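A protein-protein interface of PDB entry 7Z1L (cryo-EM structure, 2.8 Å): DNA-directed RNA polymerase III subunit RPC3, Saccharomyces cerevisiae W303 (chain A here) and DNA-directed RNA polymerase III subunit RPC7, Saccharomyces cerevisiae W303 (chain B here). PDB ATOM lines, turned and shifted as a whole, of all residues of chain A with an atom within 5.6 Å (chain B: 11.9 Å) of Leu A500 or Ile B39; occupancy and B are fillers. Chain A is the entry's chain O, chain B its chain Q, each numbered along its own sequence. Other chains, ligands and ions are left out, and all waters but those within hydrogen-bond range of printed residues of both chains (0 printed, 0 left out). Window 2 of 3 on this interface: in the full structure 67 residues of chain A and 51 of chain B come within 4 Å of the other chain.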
ATOM      1  N   VAL A 495     -17.373  15.720  -2.379  1.00  0.00           N
ATOM      2  CA  VAL A 495     -17.555  16.745  -1.352  1.00  0.00           C
ATOM      3  C   VAL A 495     -17.244  18.122  -1.924  1.00  0.00           C
ATOM      4  O   VAL A 495     -17.995  19.085  -1.711  1.00  0.00           O
ATOM      5  CB  VAL A 495     -16.692  16.431  -0.114  1.00  0.00           C
ATOM      6  CG1 VAL A 495     -16.581  17.650   0.778  1.00  0.00           C
ATOM      7  CG2 VAL A 495     -17.291  15.287   0.671  1.00  0.00           C
ATOM      8  N   ILE A 496     -16.144  18.232  -2.678  1.00  0.00           N
ATOM      9  CA  ILE A 496     -15.813  19.503  -3.323  1.00  0.00           C
ATOM     10  C   ILE A 496     -16.893  19.905  -4.324  1.00  0.00           C
ATOM     11  O   ILE A 496     -17.290  21.074  -4.391  1.00  0.00           O
ATOM     12  CB  ILE A 496     -14.424  19.429  -3.985  1.00  0.00           C
ATOM     13  CG1 ILE A 496     -13.328  19.473  -2.929  1.00  0.00           C
ATOM     14  CG2 ILE A 496     -14.224  20.552  -4.981  1.00  0.00           C
ATOM     15  CD1 ILE A 496     -11.961  19.391  -3.524  1.00  0.00           C
ATOM     16  N   ALA A 497     -17.393  18.944  -5.104  1.00  0.00           N
ATOM     17  CA  ALA A 497     -18.429  19.246  -6.088  1.00  0.00           C
ATOM     18  C   ALA A 497     -19.712  19.722  -5.422  1.00  0.00           C
ATOM     19  O   ALA A 497     -20.384  20.628  -5.926  1.00  0.00           O
ATOM     20  CB  ALA A 497     -18.707  18.019  -6.952  1.00  0.00           C
ATOM     21  N   SER A 498     -20.072  19.119  -4.290  1.00  0.00           N
ATOM     22  CA  SER A 498     -21.297  19.501  -3.604  1.00  0.00           C
ATOM     23  C   SER A 498     -21.165  20.835  -2.882  1.00  0.00           C
ATOM     24  O   SER A 498     -22.154  21.568  -2.769  1.00  0.00           O
ATOM     25  CB  SER A 498     -21.697  18.410  -2.615  1.00  0.00           C
ATOM     26  OG  SER A 498     -20.748  18.299  -1.571  1.00  0.00           O
ATOM     27  N   THR A 499     -19.974  21.172  -2.388  1.00  0.00           N
ATOM     28  CA  THR A 499     -19.814  22.419  -1.645  1.00  0.00           C
ATOM     29  C   THR A 499     -19.452  23.592  -2.554  1.00  0.00           C
ATOM     30  O   THR A 499     -20.193  24.577  -2.629  1.00  0.00           O
ATOM     31  CB  THR A 499     -18.757  22.247  -0.550  1.00  0.00           C
ATOM     32  OG1 THR A 499     -17.528  21.800  -1.137  1.00  0.00           O
ATOM     33  CG2 THR A 499     -19.223  21.235   0.476  1.00  0.00           C
ATOM     34  N   LEU A 500     -18.325  23.498  -3.252  1.00  0.00           N
ATOM     35  CA  LEU A 500     -17.810  24.598  -4.055  1.00  0.00           C
ATOM     36  C   LEU A 500     -18.311  24.586  -5.493  1.00  0.00           C
ATOM     37  O   LEU A 500     -17.935  25.470  -6.269  1.00  0.00           O
ATOM     38  CB  LEU A 500     -16.278  24.577  -4.049  1.00  0.00           C
ATOM     39  CG  LEU A 500     -15.597  24.811  -2.701  1.00  0.00           C
ATOM     40  CD1 LEU A 500     -14.100  24.593  -2.818  1.00  0.00           C
ATOM     41  CD2 LEU A 500     -15.896  26.209  -2.195  1.00  0.00           C
ATOM     42  N   GLY A 501     -19.139  23.617  -5.871  1.00  0.00           N
ATOM     43  CA  GLY A 501     -19.684  23.566  -7.206  1.00  0.00           C
ATOM     44  C   GLY A 501     -18.982  22.559  -8.096  1.00  0.00           C
ATOM     45  O   GLY A 501     -17.861  22.124  -7.817  1.00  0.00           O
ATOM     46  N   PRO A 502     -19.644  22.162  -9.187  1.00  0.00           N
ATOM     47  CA  PRO A 502     -19.032  21.180 -10.098  1.00  0.00           C
ATOM     48  C   PRO A 502     -17.813  21.707 -10.835  1.00  0.00           C
ATOM     49  O   PRO A 502     -16.948  20.913 -11.228  1.00  0.00           O
ATOM     50  CB  PRO A 502     -20.176  20.845 -11.064  1.00  0.00           C
ATOM     51  CG  PRO A 502     -21.048  22.050 -11.041  1.00  0.00           C
ATOM     52  CD  PRO A 502     -20.974  22.594  -9.645  1.00  0.00           C
ATOM     53  N   SER A 503     -17.723  23.025 -11.043  1.00  0.00           N
ATOM     54  CA  SER A 503     -16.542  23.591 -11.682  1.00  0.00           C
ATOM     55  C   SER A 503     -15.300  23.393 -10.826  1.00  0.00           C
ATOM     56  O   SER A 503     -14.200  23.206 -11.359  1.00  0.00           O
ATOM     57  CB  SER A 503     -16.757  25.077 -11.969  1.00  0.00           C
ATOM     58  OG  SER A 503     -17.749  25.263 -12.962  1.00  0.00           O
ATOM     59  N   ALA A 504     -15.457  23.418  -9.501  1.00  0.00           N
ATOM     60  CA  ALA A 504     -14.334  23.128  -8.617  1.00  0.00           C
ATOM     61  C   ALA A 504     -13.874  21.686  -8.765  1.00  0.00           C
ATOM     62  O   ALA A 504     -12.669  21.410  -8.754  1.00  0.00           O
ATOM     63  CB  ALA A 504     -14.714  23.434  -7.171  1.00  0.00           C
ATOM     64  N   SER A 539     -10.606  29.897  -4.831  1.00  0.00           N
ATOM     65  CA  SER A 539     -11.471  29.276  -3.832  1.00  0.00           C
ATOM     66  C   SER A 539     -10.909  27.936  -3.367  1.00  0.00           C
ATOM     67  O   SER A 539     -11.016  27.588  -2.186  1.00  0.00           O
ATOM     68  CB  SER A 539     -12.880  29.101  -4.393  1.00  0.00           C
ATOM     69  OG  SER A 539     -13.718  28.436  -3.465  1.00  0.00           O
ATOM     70  N   LEU A 540     -10.315  27.169  -4.284  1.00  0.00           N
ATOM     71  CA  LEU A 540      -9.779  25.858  -3.926  1.00  0.00           C
ATOM     72  C   LEU A 540      -8.519  25.963  -3.074  1.00  0.00           C
ATOM     73  O   LEU A 540      -8.209  25.037  -2.317  1.00  0.00           O
ATOM     74  CB  LEU A 540      -9.486  25.047  -5.189  1.00  0.00           C
ATOM     75  CG  LEU A 540     -10.660  24.307  -5.832  1.00  0.00           C
ATOM     76  CD1 LEU A 540     -10.288  23.840  -7.227  1.00  0.00           C
ATOM     77  CD2 LEU A 540     -11.095  23.137  -4.973  1.00  0.00           C
ATOM     78  N   TYR A 543      -8.664  25.701   1.017  1.00  0.00           N
ATOM     79  CA  TYR A 543      -8.877  24.427   1.692  1.00  0.00           C
ATOM     80  C   TYR A 543      -7.760  23.426   1.415  1.00  0.00           C
ATOM     81  O   TYR A 543      -7.984  22.216   1.521  1.00  0.00           O
ATOM     82  CB  TYR A 543     -10.228  23.837   1.290  1.00  0.00           C
ATOM     83  CG  TYR A 543     -11.359  24.835   1.321  1.00  0.00           C
ATOM     84  CD1 TYR A 543     -11.979  25.174   2.515  1.00  0.00           C
ATOM     85  CD2 TYR A 543     -11.809  25.440   0.156  1.00  0.00           C
ATOM     86  CE1 TYR A 543     -13.012  26.087   2.548  1.00  0.00           C
ATOM     87  CE2 TYR A 543     -12.841  26.354   0.181  1.00  0.00           C
ATOM     88  CZ  TYR A 543     -13.438  26.674   1.379  1.00  0.00           C
ATOM     89  OH  TYR A 543     -14.467  27.584   1.406  1.00  0.00           O
ATOM     90  N   THR B  34     -16.828  38.702   5.633  1.00  0.00           N
ATOM     91  CA  THR B  34     -17.883  38.177   6.483  1.00  0.00           C
ATOM     92  C   THR B  34     -17.314  37.218   7.522  1.00  0.00           C
ATOM     93  O   THR B  34     -16.274  36.586   7.321  1.00  0.00           O
ATOM     94  CB  THR B  34     -18.951  37.477   5.642  1.00  0.00           C
ATOM     95  OG1 THR B  34     -20.015  37.029   6.491  1.00  0.00           O
ATOM     96  CG2 THR B  34     -18.364  36.291   4.891  1.00  0.00           C
ATOM     97  N   GLU B  35     -18.001  37.138   8.656  1.00  0.00           N
ATOM     98  CA  GLU B  35     -17.632  36.238   9.736  1.00  0.00           C
ATOM     99  C   GLU B  35     -18.493  34.982   9.746  1.00  0.00           C
ATOM    100  O   GLU B  35     -18.145  34.003  10.414  1.00  0.00           O
ATOM    101  CB  GLU B  35     -17.739  36.976  11.079  1.00  0.00           C
ATOM    102  CG  GLU B  35     -17.084  36.285  12.263  1.00  0.00           C
ATOM    103  CD  GLU B  35     -15.573  36.267  12.162  1.00  0.00           C
ATOM    104  OE1 GLU B  35     -15.008  37.175  11.519  1.00  0.00           O
ATOM    105  OE2 GLU B  35     -14.950  35.343  12.725  1.00  0.00           O
ATOM    106  N   PHE B  36     -19.588  34.976   8.991  1.00  0.00           N
ATOM    107  CA  PHE B  36     -20.526  33.875   8.964  1.00  0.00           C
ATOM    108  C   PHE B  36     -20.373  33.099   7.663  1.00  0.00           C
ATOM    109  O   PHE B  36     -20.337  33.707   6.584  1.00  0.00           O
ATOM    110  CB  PHE B  36     -21.962  34.392   9.105  1.00  0.00           C
ATOM    111  CG  PHE B  36     -22.182  35.229  10.332  1.00  0.00           C
ATOM    112  CD1 PHE B  36     -22.486  34.637  11.545  1.00  0.00           C
ATOM    113  CD2 PHE B  36     -22.078  36.608  10.273  1.00  0.00           C
ATOM    114  CE1 PHE B  36     -22.686  35.403  12.674  1.00  0.00           C
ATOM    115  CE2 PHE B  36     -22.276  37.380  11.399  1.00  0.00           C
ATOM    116  CZ  PHE B  36     -22.580  36.775  12.601  1.00  0.00           C
ATOM    117  N   PRO B  37     -20.279  31.774   7.718  1.00  0.00           N
ATOM    118  CA  PRO B  37     -20.059  30.995   6.496  1.00  0.00           C
ATOM    119  C   PRO B  37     -21.303  30.939   5.623  1.00  0.00           C
ATOM    120  O   PRO B  37     -22.422  31.220   6.056  1.00  0.00           O
ATOM    121  CB  PRO B  37     -19.693  29.606   7.027  1.00  0.00           C
ATOM    122  CG  PRO B  37     -20.360  29.538   8.356  1.00  0.00           C
ATOM    123  CD  PRO B  37     -20.331  30.925   8.920  1.00  0.00           C
ATOM    124  N   SER B  38     -21.085  30.565   4.359  1.00  0.00           N
ATOM    125  CA  SER B  38     -22.172  30.513   3.391  1.00  0.00           C
ATOM    126  C   SER B  38     -22.129  29.274   2.502  1.00  0.00           C
ATOM    127  O   SER B  38     -22.861  29.224   1.505  1.00  0.00           O
ATOM    128  CB  SER B  38     -22.161  31.770   2.513  1.00  0.00           C
ATOM    129  OG  SER B  38     -22.309  32.940   3.299  1.00  0.00           O
ATOM    130  N   ILE B  39     -21.307  28.280   2.821  1.00  0.00           N
ATOM    131  CA  ILE B  39     -21.177  27.085   1.990  1.00  0.00           C
ATOM    132  C   ILE B  39     -21.584  25.865   2.809  1.00  0.00           C
ATOM    133  O   ILE B  39     -20.751  25.297   3.530  1.00  0.00           O
ATOM    134  CB  ILE B  39     -19.748  26.937   1.447  1.00  0.00           C
ATOM    135  CG1 ILE B  39     -19.275  28.249   0.819  1.00  0.00           C
ATOM    136  CG2 ILE B  39     -19.678  25.812   0.431  1.00  0.00           C
ATOM    137  CD1 ILE B  39     -17.871  28.194   0.271  1.00  0.00           C
ATOM    138  N   PRO B  40     -22.837  25.430   2.733  1.00  0.00           N
ATOM    139  CA  PRO B  40     -23.284  24.312   3.568  1.00  0.00           C
ATOM    140  C   PRO B  40     -23.040  22.958   2.923  1.00  0.00           C
ATOM    141  O   PRO B  40     -23.085  22.798   1.701  1.00  0.00           O
ATOM    142  CB  PRO B  40     -24.785  24.578   3.721  1.00  0.00           C
ATOM    143  CG  PRO B  40     -25.159  25.259   2.449  1.00  0.00           C
ATOM    144  CD  PRO B  40     -23.951  26.044   1.990  1.00  0.00           C
ATOM    145  N   LEU B  41     -22.770  21.975   3.779  1.00  0.00           N
ATOM    146  CA  LEU B  41     -22.684  20.593   3.347  1.00  0.00           C
ATOM    147  C   LEU B  41     -24.085  20.048   3.067  1.00  0.00           C
ATOM    148  O   LEU B  41     -25.070  20.533   3.628  1.00  0.00           O
ATOM    149  CB  LEU B  41     -21.982  19.756   4.417  1.00  0.00           C
ATOM    150  CG  LEU B  41     -20.454  19.738   4.364  1.00  0.00           C
ATOM    151  CD1 LEU B  41     -19.876  19.327   5.705  1.00  0.00           C
ATOM    152  CD2 LEU B  41     -19.966  18.810   3.268  1.00  0.00           C
ATOM    153  N   PRO B  42     -24.206  19.033   2.203  1.00  0.00           N
ATOM    154  CA  PRO B  42     -25.538  18.502   1.868  1.00  0.00           C
ATOM    155  C   PRO B  42     -26.160  17.628   2.945  1.00  0.00           C
ATOM    156  O   PRO B  42     -27.156  16.952   2.664  1.00  0.00           O
ATOM    157  CB  PRO B  42     -25.283  17.678   0.595  1.00  0.00           C
ATOM    158  CG  PRO B  42     -23.907  18.010   0.161  1.00  0.00           C
ATOM    159  CD  PRO B  42     -23.158  18.423   1.371  1.00  0.00           C
ATOM    160  N   ILE B  43     -25.619  17.616   4.159  1.00  0.00           N
ATOM    161  CA  ILE B  43     -26.091  16.735   5.219  1.00  0.00           C
ATOM    162  C   ILE B  43     -27.280  17.357   5.937  1.00  0.00           C
ATOM    163  O   ILE B  43     -27.871  16.740   6.830  1.00  0.00           O
ATOM    164  CB  ILE B  43     -24.963  16.451   6.220  1.00  0.00           C
ATOM    165  CG1 ILE B  43     -24.538  17.761   6.867  1.00  0.00           C
ATOM    166  CG2 ILE B  43     -23.782  15.808   5.522  1.00  0.00           C
ATOM    167  CD1 ILE B  43     -23.513  17.604   7.916  1.00  0.00           C
ATOM    168  N   ASN B  44     -27.639  18.583   5.562  1.00  0.00           N
ATOM    169  CA  ASN B  44     -28.621  19.362   6.306  1.00  0.00           C
ATOM    170  C   ASN B  44     -30.048  19.143   5.817  1.00  0.00           C
ATOM    171  O   ASN B  44     -30.900  20.024   5.988  1.00  0.00           O
ATOM    172  CB  ASN B  44     -28.255  20.844   6.247  1.00  0.00           C
ATOM    173  CG  ASN B  44     -26.768  21.080   6.402  1.00  0.00           C
ATOM    174  OD1 ASN B  44     -26.146  21.753   5.581  1.00  0.00           O
ATOM    175  ND2 ASN B  44     -26.188  20.528   7.458  1.00  0.00           N
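OG of Ser A498 sits at hydrogen-bond distance from O of Val A495, 2.9 Å away.
OG1 of Thr A499 sits at hydrogen-bond distance from O of Val A495 (2.8 Å).
The backbone carbonyl oxygen (O) of Ile A496 sits at hydrogen-bond distance from the side-chain hydroxyl (OG1) of Thr A499 (3.3 Å).
O of Leu B41 lies close to OD1 of Asn B44, at 2.5 Å.
Of chain B, only Ile B39 comes within 4 Å of Leu A500.
Ile A496 touches none of the printed residues of chain B.
No residue of chain B comes within 4 Å of Ala A497.
Of the printed residues of chain B, Ser A498 touches Pro B42.
Thr A499 touches two residues of chain B.
No residue of chain B comes within 4 Å of Gly A501.
No residue of chain B comes within 4 Å of Pro A502.
No residue of chain B comes within 4 Å of Ser A503.
No residue of chain B comes within 4 Å of Ala A504.
No residue of chain B comes within 4 Å of Ser A539.
No residue of chain B comes within 4 Å of Leu A540.
Printed residues of chain B within 4 Å of Tyr A543: Ile B39.
Of the printed residues of chain A, Pro B42 touches Ser A498 (3.6 Å).
Ile B43 touches none of the printed residues of chain A.
The nearest printed residue of chain A that does not touch Ile B39 is Ser A539 (5.6 Å).
Ser A498 touches Pro B42.
Ile B39 touches Thr A499 (CG2 to O, 3.3 Å).
Thr A499 touches Leu B41.
Ile B39 touches Leu A500 (CD1 to CD2, 3.7 Å).
OH of Tyr A543 touches CD1 of Ile B39, at 3.6 Å.
Of the 11 printed residues of chain B, 3 touch a printed residue of chain A.
Hydrophobic or aromatic side chains of chain B within 4 Å of the printed part of chain A: Ile B39, Leu B41 and Pro B42.
Of the 13 printed residues of chain A, 4 touch a printed residue of chain B.
Along chain A the printed residues that touch a printed residue of chain B span positions 498 to 543.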
